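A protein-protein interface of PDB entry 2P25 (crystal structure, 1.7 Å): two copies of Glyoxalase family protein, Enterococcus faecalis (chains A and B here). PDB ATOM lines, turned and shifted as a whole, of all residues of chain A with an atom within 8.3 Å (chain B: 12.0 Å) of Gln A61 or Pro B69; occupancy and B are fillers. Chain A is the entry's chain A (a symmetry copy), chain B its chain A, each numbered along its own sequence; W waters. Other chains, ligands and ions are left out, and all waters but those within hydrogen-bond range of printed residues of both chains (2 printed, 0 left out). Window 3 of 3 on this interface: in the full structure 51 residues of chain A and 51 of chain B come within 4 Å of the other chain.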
ATOM      1  N   ASN A  12       5.395 -12.527 -24.011  1.00  0.00           N
ATOM      2  CA  ASN A  12       4.047 -12.189 -24.523  1.00  0.00           C
ATOM      3  C   ASN A  12       3.027 -12.760 -23.543  1.00  0.00           C
ATOM      4  O   ASN A  12       3.093 -13.949 -23.231  1.00  0.00           O
ATOM      5  CB  ASN A  12       3.799 -12.822 -25.917  1.00  0.00           C
ATOM      6  CG  ASN A  12       4.675 -12.225 -27.007  1.00  0.00           C
ATOM      7  OD1 ASN A  12       5.163 -11.105 -26.868  1.00  0.00           O
ATOM      8  ND2 ASN A  12       4.869 -12.972 -28.117  1.00  0.00           N
ATOM      9  N   ALA A  13       2.123 -11.900 -23.056  1.00  0.00           N
ATOM     10  CA  ALA A  13       1.112 -12.269 -22.074  1.00  0.00           C
ATOM     11  C   ALA A  13      -0.262 -11.862 -22.585  1.00  0.00           C
ATOM     12  O   ALA A  13      -0.376 -10.941 -23.431  1.00  0.00           O
ATOM     13  CB  ALA A  13       1.384 -11.570 -20.725  1.00  0.00           C
ATOM     14  N   SER A  14      -1.309 -12.498 -22.038  1.00  0.00           N
ATOM     15  CA  SER A  14      -2.665 -12.263 -22.587  1.00  0.00           C
ATOM     16  C   SER A  14      -3.484 -11.211 -21.850  1.00  0.00           C
ATOM     17  O   SER A  14      -4.354 -10.568 -22.443  1.00  0.00           O
ATOM     18  CB  SER A  14      -3.487 -13.559 -22.599  1.00  0.00           C
ATOM     19  OG  SER A  14      -3.696 -13.990 -21.266  1.00  0.00           O
ATOM     20  N   ASN A  15      -3.237 -11.046 -20.558  1.00  0.00           N
ATOM     21  CA  ASN A  15      -4.152 -10.271 -19.727  1.00  0.00           C
ATOM     22  C   ASN A  15      -3.412  -9.344 -18.780  1.00  0.00           C
ATOM     23  O   ASN A  15      -2.515  -9.769 -18.050  1.00  0.00           O
ATOM     24  CB  ASN A  15      -5.035 -11.253 -18.940  1.00  0.00           C
ATOM     25  CG  ASN A  15      -6.049 -10.551 -18.028  1.00  0.00           C
ATOM     26  OD1 ASN A  15      -5.750 -10.181 -16.877  1.00  0.00           O
ATOM     27  ND2 ASN A  15      -7.251 -10.379 -18.541  1.00  0.00           N
ATOM     28  N   LYS A  40      -0.471  -1.338 -32.221  1.00  0.00           N
ATOM     29  CA  LYS A  40       0.127  -2.679 -32.163  1.00  0.00           C
ATOM     30  C   LYS A  40      -0.593  -3.953 -31.720  1.00  0.00           C
ATOM     31  O   LYS A  40       0.015  -5.017 -31.782  1.00  0.00           O
ATOM     32  CB  LYS A  40       1.574  -2.617 -31.659  1.00  0.00           C
ATOM     33  CG  LYS A  40       2.541  -2.390 -32.816  1.00  0.00           C
ATOM     34  CD  LYS A  40       3.920  -2.008 -32.354  1.00  0.00           C
ATOM     35  CE  LYS A  40       4.864  -1.826 -33.537  1.00  0.00           C
ATOM     36  NZ  LYS A  40       6.132  -1.142 -33.126  1.00  0.00           N
ATOM     37  N   ASN A  41      -1.816  -3.916 -31.196  1.00  0.00           N
ATOM     38  CA  ASN A  41      -2.323  -2.922 -30.312  1.00  0.00           C
ATOM     39  C   ASN A  41      -2.176  -3.642 -28.967  1.00  0.00           C
ATOM     40  O   ASN A  41      -2.817  -4.672 -28.682  1.00  0.00           O
ATOM     41  CB  ASN A  41      -3.785  -2.621 -30.600  1.00  0.00           C
ATOM     42  CG  ASN A  41      -4.681  -3.857 -30.486  1.00  0.00           C
ATOM     43  OD1 ASN A  41      -4.275  -4.986 -30.795  1.00  0.00           O
ATOM     44  ND2 ASN A  41      -5.908  -3.639 -30.034  1.00  0.00           N
ATOM     45  N   ASP A  42      -1.263  -3.142 -28.163  1.00  0.00           N
ATOM     46  CA  ASP A  42      -0.884  -3.882 -26.987  1.00  0.00           C
ATOM     47  C   ASP A  42      -0.518  -2.907 -25.902  1.00  0.00           C
ATOM     48  O   ASP A  42      -0.674  -1.686 -26.067  1.00  0.00           O
ATOM     49  CB  ASP A  42       0.254  -4.888 -27.297  1.00  0.00           C
ATOM     50  CG  ASP A  42       1.525  -4.232 -27.848  1.00  0.00           C
ATOM     51  OD1 ASP A  42       1.685  -3.002 -27.737  1.00  0.00           O
ATOM     52  OD2 ASP A  42       2.388  -4.963 -28.390  1.00  0.00           O
ATOM     53  N   ILE A  58       1.512  -7.206 -23.752  1.00  0.00           N
ATOM     54  CA  ILE A  58       0.239  -7.751 -23.311  1.00  0.00           C
ATOM     55  C   ILE A  58      -0.817  -7.517 -24.388  1.00  0.00           C
ATOM     56  O   ILE A  58      -1.085  -6.387 -24.755  1.00  0.00           O
ATOM     57  CB  ILE A  58      -0.235  -7.087 -21.975  1.00  0.00           C
ATOM     58  CG1 ILE A  58       0.868  -7.180 -20.905  1.00  0.00           C
ATOM     59  CG2 ILE A  58      -1.524  -7.738 -21.445  1.00  0.00           C
ATOM     60  CD1 ILE A  58       0.661  -6.273 -19.731  1.00  0.00           C
ATOM     61  N   SER A  59      -1.447  -8.585 -24.845  1.00  0.00           N
ATOM     62  CA  SER A  59      -2.417  -8.496 -25.953  1.00  0.00           C
ATOM     63  C   SER A  59      -3.282  -9.750 -26.000  1.00  0.00           C
ATOM     64  O   SER A  59      -2.791 -10.859 -25.809  1.00  0.00           O
ATOM     65  CB  SER A  59      -1.690  -8.323 -27.288  1.00  0.00           C
ATOM     66  OG  SER A  59      -2.606  -8.266 -28.384  1.00  0.00           O
ATOM     67  N   ASP A  60      -4.554  -9.577 -26.336  1.00  0.00           N
ATOM     68  CA  ASP A  60      -5.402 -10.743 -26.536  1.00  0.00           C
ATOM     69  C   ASP A  60      -5.215 -11.361 -27.925  1.00  0.00           C
ATOM     70  O   ASP A  60      -5.904 -12.308 -28.273  1.00  0.00           O
ATOM     71  CB  ASP A  60      -6.875 -10.411 -26.256  1.00  0.00           C
ATOM     72  CG  ASP A  60      -7.446  -9.430 -27.244  1.00  0.00           C
ATOM     73  OD1 ASP A  60      -6.696  -8.917 -28.096  1.00  0.00           O
ATOM     74  OD2 ASP A  60      -8.673  -9.164 -27.166  1.00  0.00           O
ATOM     75  N   GLN A  61      -4.272 -10.855 -28.704  1.00  0.00           N
ATOM     76  CA  GLN A  61      -4.066 -11.367 -30.064  1.00  0.00           C
ATOM     77  C   GLN A  61      -3.175 -12.613 -30.131  1.00  0.00           C
ATOM     78  O   GLN A  61      -3.180 -13.358 -31.143  1.00  0.00           O
ATOM     79  CB  GLN A  61      -3.536 -10.261 -30.971  1.00  0.00           C
ATOM     80  CG  GLN A  61      -4.589  -9.159 -31.171  1.00  0.00           C
ATOM     81  CD  GLN A  61      -5.811  -9.655 -31.948  1.00  0.00           C
ATOM     82  OE1 GLN A  61      -6.876  -9.922 -31.373  1.00  0.00           O
ATOM     83  NE2 GLN A  61      -5.646  -9.817 -33.255  1.00  0.00           N
ATOM     84  N   PHE A  62      -2.408 -12.847 -29.073  1.00  0.00           N
ATOM     85  CA  PHE A  62      -1.455 -13.949 -29.086  1.00  0.00           C
ATOM     86  C   PHE A  62      -2.176 -15.274 -28.812  1.00  0.00           C
ATOM     87  O   PHE A  62      -2.802 -15.422 -27.774  1.00  0.00           O
ATOM     88  CB  PHE A  62      -0.404 -13.764 -27.987  1.00  0.00           C
ATOM     89  CG  PHE A  62       0.330 -12.451 -28.016  1.00  0.00           C
ATOM     90  CD1 PHE A  62       0.969 -12.002 -29.162  1.00  0.00           C
ATOM     91  CD2 PHE A  62       0.423 -11.687 -26.850  1.00  0.00           C
ATOM     92  CE1 PHE A  62       1.676 -10.788 -29.159  1.00  0.00           C
ATOM     93  CE2 PHE A  62       1.149 -10.487 -26.829  1.00  0.00           C
ATOM     94  CZ  PHE A  62       1.764 -10.030 -27.961  1.00  0.00           C
ATOM     95  N   PRO A  63      -2.020 -16.274 -29.706  1.00  0.00           N
ATOM     96  CA  PRO A  63      -2.544 -17.608 -29.417  1.00  0.00           C
ATOM     97  C   PRO A  63      -1.703 -18.343 -28.364  1.00  0.00           C
ATOM     98  O   PRO A  63      -0.616 -17.879 -27.983  1.00  0.00           O
ATOM     99  CB  PRO A  63      -2.423 -18.332 -30.775  1.00  0.00           C
ATOM    100  CG  PRO A  63      -1.243 -17.689 -31.399  1.00  0.00           C
ATOM    101  CD  PRO A  63      -1.354 -16.224 -31.021  1.00  0.00           C
ATOM    102  N   ALA A  64      -2.198 -19.499 -27.942  1.00  0.00           N
ATOM    103  CA  ALA A  64      -1.570 -20.282 -26.880  1.00  0.00           C
ATOM    104  C   ALA A  64      -0.121 -20.629 -27.193  1.00  0.00           C
ATOM    105  O   ALA A  64       0.247 -20.872 -28.343  1.00  0.00           O
ATOM    106  CB  ALA A  64      -2.356 -21.570 -26.638  1.00  0.00           C
ATOM    107  N   PRO B  63       8.249 -27.750 -34.286  1.00  0.00           N
ATOM    108  CA  PRO B  63       7.781 -26.963 -35.427  1.00  0.00           C
ATOM    109  C   PRO B  63       8.252 -25.505 -35.354  1.00  0.00           C
ATOM    110  O   PRO B  63       8.801 -25.065 -34.331  1.00  0.00           O
ATOM    111  CB  PRO B  63       6.246 -27.021 -35.284  1.00  0.00           C
ATOM    112  CG  PRO B  63       6.045 -27.123 -33.819  1.00  0.00           C
ATOM    113  CD  PRO B  63       7.157 -28.035 -33.338  1.00  0.00           C
ATOM    114  N   ALA B  64       7.991 -24.765 -36.425  1.00  0.00           N
ATOM    115  CA  ALA B  64       8.448 -23.384 -36.555  1.00  0.00           C
ATOM    116  C   ALA B  64       7.968 -22.502 -35.411  1.00  0.00           C
ATOM    117  O   ALA B  64       6.861 -22.666 -34.895  1.00  0.00           O
ATOM    118  CB  ALA B  64       7.971 -22.794 -37.882  1.00  0.00           C
ATOM    119  N   ARG B  65       8.801 -21.542 -35.051  1.00  0.00           N
ATOM    120  CA  ARG B  65       8.430 -20.558 -34.042  1.00  0.00           C
ATOM    121  C   ARG B  65       7.228 -19.764 -34.602  1.00  0.00           C
ATOM    122  O   ARG B  65       7.301 -19.210 -35.702  1.00  0.00           O
ATOM    123  CB  ARG B  65       9.610 -19.619 -33.820  1.00  0.00           C
ATOM    124  CG  ARG B  65       9.297 -18.525 -32.794  1.00  0.00           C
ATOM    125  CD  ARG B  65      10.479 -17.561 -32.666  1.00  0.00           C
ATOM    126  NE  ARG B  65      10.186 -16.499 -31.710  1.00  0.00           N
ATOM    127  CZ  ARG B  65       9.597 -15.349 -32.020  1.00  0.00           C
ATOM    128  NH1 ARG B  65       9.198 -15.112 -33.269  1.00  0.00           N
ATOM    129  NH2 ARG B  65       9.394 -14.439 -31.067  1.00  0.00           N
ATOM    130  N   PRO B  66       6.109 -19.730 -33.866  1.00  0.00           N
ATOM    131  CA  PRO B  66       4.947 -18.963 -34.366  1.00  0.00           C
ATOM    132  C   PRO B  66       5.245 -17.495 -34.607  1.00  0.00           C
ATOM    133  O   PRO B  66       5.977 -16.869 -33.865  1.00  0.00           O
ATOM    134  CB  PRO B  66       3.915 -19.105 -33.243  1.00  0.00           C
ATOM    135  CG  PRO B  66       4.252 -20.406 -32.611  1.00  0.00           C
ATOM    136  CD  PRO B  66       5.780 -20.442 -32.616  1.00  0.00           C
ATOM    137  N   SER B  67       4.680 -16.971 -35.691  1.00  0.00           N
ATOM    138  CA  SER B  67       4.772 -15.557 -35.973  1.00  0.00           C
ATOM    139  C   SER B  67       3.507 -15.157 -36.733  1.00  0.00           C
ATOM    140  O   SER B  67       2.807 -16.008 -37.315  1.00  0.00           O
ATOM    141  CB  SER B  67       6.060 -15.247 -36.758  1.00  0.00           C
ATOM    142  OG  SER B  67       6.036 -15.911 -38.031  1.00  0.00           O
ATOM    143  N   TYR B  68       3.171 -13.872 -36.682  1.00  0.00           N
ATOM    144  CA  TYR B  68       2.022 -13.360 -37.446  1.00  0.00           C
ATOM    145  C   TYR B  68       0.710 -14.129 -37.210  1.00  0.00           C
ATOM    146  O   TYR B  68       0.091 -14.654 -38.136  1.00  0.00           O
ATOM    147  CB  TYR B  68       2.402 -13.247 -38.949  1.00  0.00           C
ATOM    148  CG  TYR B  68       3.602 -12.340 -39.121  1.00  0.00           C
ATOM    149  CD1 TYR B  68       3.456 -10.951 -39.093  1.00  0.00           C
ATOM    150  CD2 TYR B  68       4.892 -12.868 -39.259  1.00  0.00           C
ATOM    151  CE1 TYR B  68       4.572 -10.098 -39.215  1.00  0.00           C
ATOM    152  CE2 TYR B  68       6.005 -12.033 -39.380  1.00  0.00           C
ATOM    153  CZ  TYR B  68       5.828 -10.648 -39.350  1.00  0.00           C
ATOM    154  OH  TYR B  68       6.926  -9.832 -39.471  1.00  0.00           O
ATOM    155  N   PRO B  69       0.248 -14.176 -35.959  1.00  0.00           N
ATOM    156  CA  PRO B  69       0.810 -13.553 -34.755  1.00  0.00           C
ATOM    157  C   PRO B  69       1.802 -14.438 -33.984  1.00  0.00           C
ATOM    158  O   PRO B  69       1.768 -15.669 -34.086  1.00  0.00           O
ATOM    159  CB  PRO B  69      -0.442 -13.349 -33.893  1.00  0.00           C
ATOM    160  CG  PRO B  69      -1.277 -14.583 -34.196  1.00  0.00           C
ATOM    161  CD  PRO B  69      -1.058 -14.821 -35.692  1.00  0.00           C
ATOM    162  N   GLU B  70       2.664 -13.805 -33.204  1.00  0.00           N
ATOM    163  CA  GLU B  70       3.467 -14.556 -32.239  1.00  0.00           C
ATOM    164  C   GLU B  70       2.565 -15.175 -31.165  1.00  0.00           C
ATOM    165  O   GLU B  70       1.437 -14.735 -30.932  1.00  0.00           O
ATOM    166  CB  GLU B  70       4.501 -13.667 -31.591  1.00  0.00           C
ATOM    167  CG  GLU B  70       5.684 -13.321 -32.497  1.00  0.00           C
ATOM    168  CD  GLU B  70       6.682 -12.446 -31.783  1.00  0.00           C
ATOM    169  OE1 GLU B  70       6.300 -11.895 -30.727  1.00  0.00           O
ATOM    170  OE2 GLU B  70       7.836 -12.300 -32.260  1.00  0.00           O
ATOM    171  N   ALA B  71       3.080 -16.206 -30.510  1.00  0.00           N
ATOM    172  CA  ALA B  71       2.303 -16.876 -29.493  1.00  0.00           C
ATOM    173  C   ALA B  71       2.698 -16.343 -28.106  1.00  0.00           C
ATOM    174  O   ALA B  71       3.751 -15.708 -27.911  1.00  0.00           O
ATOM    175  CB  ALA B  71       2.537 -18.383 -29.569  1.00  0.00           C
ATOM    176  N   LEU B  72       1.825 -16.614 -27.166  1.00  0.00           N
ATOM    177  CA  LEU B  72       2.141 -16.421 -25.759  1.00  0.00           C
ATOM    178  C   LEU B  72       3.433 -17.128 -25.387  1.00  0.00           C
ATOM    179  O   LEU B  72       3.767 -18.194 -25.952  1.00  0.00           O
ATOM    180  CB  LEU B  72       0.971 -16.947 -24.924  1.00  0.00           C
ATOM    181  CG  LEU B  72      -0.302 -16.108 -25.087  1.00  0.00           C
ATOM    182  CD1 LEU B  72      -1.490 -16.863 -24.515  1.00  0.00           C
ATOM    183  CD2 LEU B  72      -0.131 -14.721 -24.405  1.00  0.00           C
ATOM    184  N   GLY B  73       4.151 -16.538 -24.428  1.00  0.00           N
ATOM    185  CA  GLY B  73       5.367 -17.147 -23.881  1.00  0.00           C
ATOM    186  C   GLY B  73       6.565 -16.261 -24.126  1.00  0.00           C
ATOM    187  O   GLY B  73       6.441 -15.056 -24.282  1.00  0.00           O
ATOM    188  N   LEU B  74       7.749 -16.853 -24.124  1.00  0.00           N
ATOM    189  CA  LEU B  74       8.967 -16.041 -24.323  1.00  0.00           C
ATOM    190  C   LEU B  74       9.079 -15.568 -25.771  1.00  0.00           C
ATOM    191  O   LEU B  74       8.888 -16.347 -26.702  1.00  0.00           O
ATOM    192  CB  LEU B  74      10.169 -16.860 -23.911  1.00  0.00           C
ATOM    193  CG  LEU B  74      10.338 -16.964 -22.385  1.00  0.00           C
ATOM    194  CD1 LEU B  74      11.229 -18.165 -22.020  1.00  0.00           C
ATOM    195  CD2 LEU B  74      10.948 -15.647 -21.854  1.00  0.00           C
ATOM    196  N   ARG B  75       9.373 -14.282 -25.938  1.00  0.00           N
ATOM    197  CA  ARG B  75       9.348 -13.617 -27.241  1.00  0.00           C
ATOM    198  C   ARG B  75      10.755 -13.397 -27.822  1.00  0.00           C
ATOM    199  O   ARG B  75      11.038 -13.751 -28.968  1.00  0.00           O
ATOM    200  CB  ARG B  75       8.662 -12.242 -27.074  1.00  0.00           C
ATOM    201  CG  ARG B  75       8.612 -11.393 -28.321  1.00  0.00           C
ATOM    202  CD  ARG B  75       7.971 -10.069 -27.902  1.00  0.00           C
ATOM    203  NE  ARG B  75       7.824  -9.093 -28.969  1.00  0.00           N
ATOM    204  CZ  ARG B  75       6.655  -8.567 -29.368  1.00  0.00           C
ATOM    205  NH1 ARG B  75       5.474  -8.953 -28.848  1.00  0.00           N
ATOM    206  NH2 ARG B  75       6.665  -7.664 -30.337  1.00  0.00           N
ATOM    207  N   GLY B 119      15.217 -18.515 -36.585  1.00  0.00           N
ATOM    208  CA  GLY B 119      14.402 -17.289 -36.622  1.00  0.00           C
ATOM    209  C   GLY B 119      14.054 -16.689 -35.268  1.00  0.00           C
ATOM    210  O   GLY B 119      13.146 -15.842 -35.183  1.00  0.00           O
ATOM    211  N   PRO B 121      14.187 -14.077 -32.611  1.00  0.00           N
ATOM    212  CA  PRO B 121      14.705 -12.695 -32.544  1.00  0.00           C
ATOM    213  C   PRO B 121      15.642 -12.481 -31.366  1.00  0.00           C
ATOM    214  O   PRO B 121      15.324 -12.836 -30.206  1.00  0.00           O
ATOM    215  CB  PRO B 121      13.430 -11.828 -32.389  1.00  0.00           C
ATOM    216  CG  PRO B 121      12.271 -12.764 -32.785  1.00  0.00           C
ATOM    217  CD  PRO B 121      12.735 -14.133 -32.369  1.00  0.00           C
HETATM  218  O   HOH W   1       3.546 -16.024 -21.213  1.00  0.00           O
HETATM  219  O   HOH W   2       3.272  -7.279 -29.791  1.00  0.00           O
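The side-chain amide oxygen (OD1) of Asn A12 lies within hydrogen-bond range of the guanidinium group (NH1) of Arg B75 (2.9 Å). N of Leu B72 sits at hydrogen-bond distance from O of Pro A63, at 2.9 Å. The backbone carbonyl oxygen (O) of Ala B71 lies within hydrogen-bond range of the side-chain amide nitrogen (ND2) of Asn A12 (3.0 Å). O of Gly B73 sits at hydrogen-bond distance from N of Asn A12. ND2 of Asn A12 lies within hydrogen-bond range of OE1 of Glu B70 (3.2 Å).
The backbone carbonyl oxygen of Arg B75 sits at hydrogen-bond distance from the guanidinium group of Arg B65 (2.8 Å). The guanidinium group (NH2) of Arg B65 is in salt-bridge range of the side-chain carboxylate (OE2) of Glu B70 (2.9 Å). The side-chain hydroxyl (OG) of Ser A59 lies close to the backbone NH (N) of Gln A61 (3.1 Å). The side-chain carboxylate of Asp A60 sits close to the side-chain amide oxygen of Gln A61. The side-chain carboxylate (OE1) of Glu B70 is in salt-bridge range of the guanidinium group (NH1) of Arg B75 (3.6 Å). The backbone carbonyl oxygen of Ala A13 is in hydrogen-bond range of the backbone NH of Ser A59, at 2.9 Å.
Among the printed residues, merely in contact across the chains: Pro A63 with Glu B70, Phe A62 with Glu B70, Ala A13 with Leu B72, Pro A63 with Ala B71, Ser A14 with Leu B72, Asn A12 with Leu B72, Pro A63 with Pro B69, Ala A64 with Ala B71, Phe A62 with Leu B72, Gln A61 with Pro B69 and Phe A62 with Arg B75.
Gln A61 touches one residue of chain B. Pro B69 touches two residues of chain A. No residue of chain B comes within 4 Å of Asn A41. No residue of chain B comes within 4 Å of Asp A60. Printed residues of chain B within 4 Å of Ser A14: Leu B72 (3.5 Å). Printed residues of chain A within 4 Å of Glu B70: Asn A12 (3.2 Å), Phe A62 (3.3 Å) and Pro A63 (3.2 Å). Of the printed residues of chain A, Leu B72 touches Asn A12, Ala A13, Ser A14, Phe A62 and Pro A63. Of the printed residues of chain B, Ala A64 touches Ala B71 (3.6 Å). Of the printed residues of chain A, Gly B73 touches Asn A12. The nearest residue of chain B that does not touch Gln A61 is Glu B70 (4.8 Å). The nearest residue of chain A that does not touch Pro B69 is Phe A62 (4.9 Å).
Printed residues of chain B that touch a printed residue of chain A: Pro B69, Glu B70, Ala B71, Leu B72, Gly B73 and Arg B75. Hydrophobic or aromatic side chains of chain B within 4 Å of the printed part of chain A: Pro B69, Ala B71 and Leu B72. Hydrophobic or aromatic side chains of chain A within 4 Å of the printed part of chain B: Phe A62 and Pro A63. Among the printed residues, 16 pairs touch across the chains.
Positions printed for both chains: 63 and 64.
Water W2 lies within hydrogen-bond range of OD2 of Asp A42 (2.8 Å) and NH1 of Arg B75 (2.9 Å). Water W1 lies within hydrogen-bond range of O of Asn A12 (2.9 Å) and N of Gly B73 (3.3 Å).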
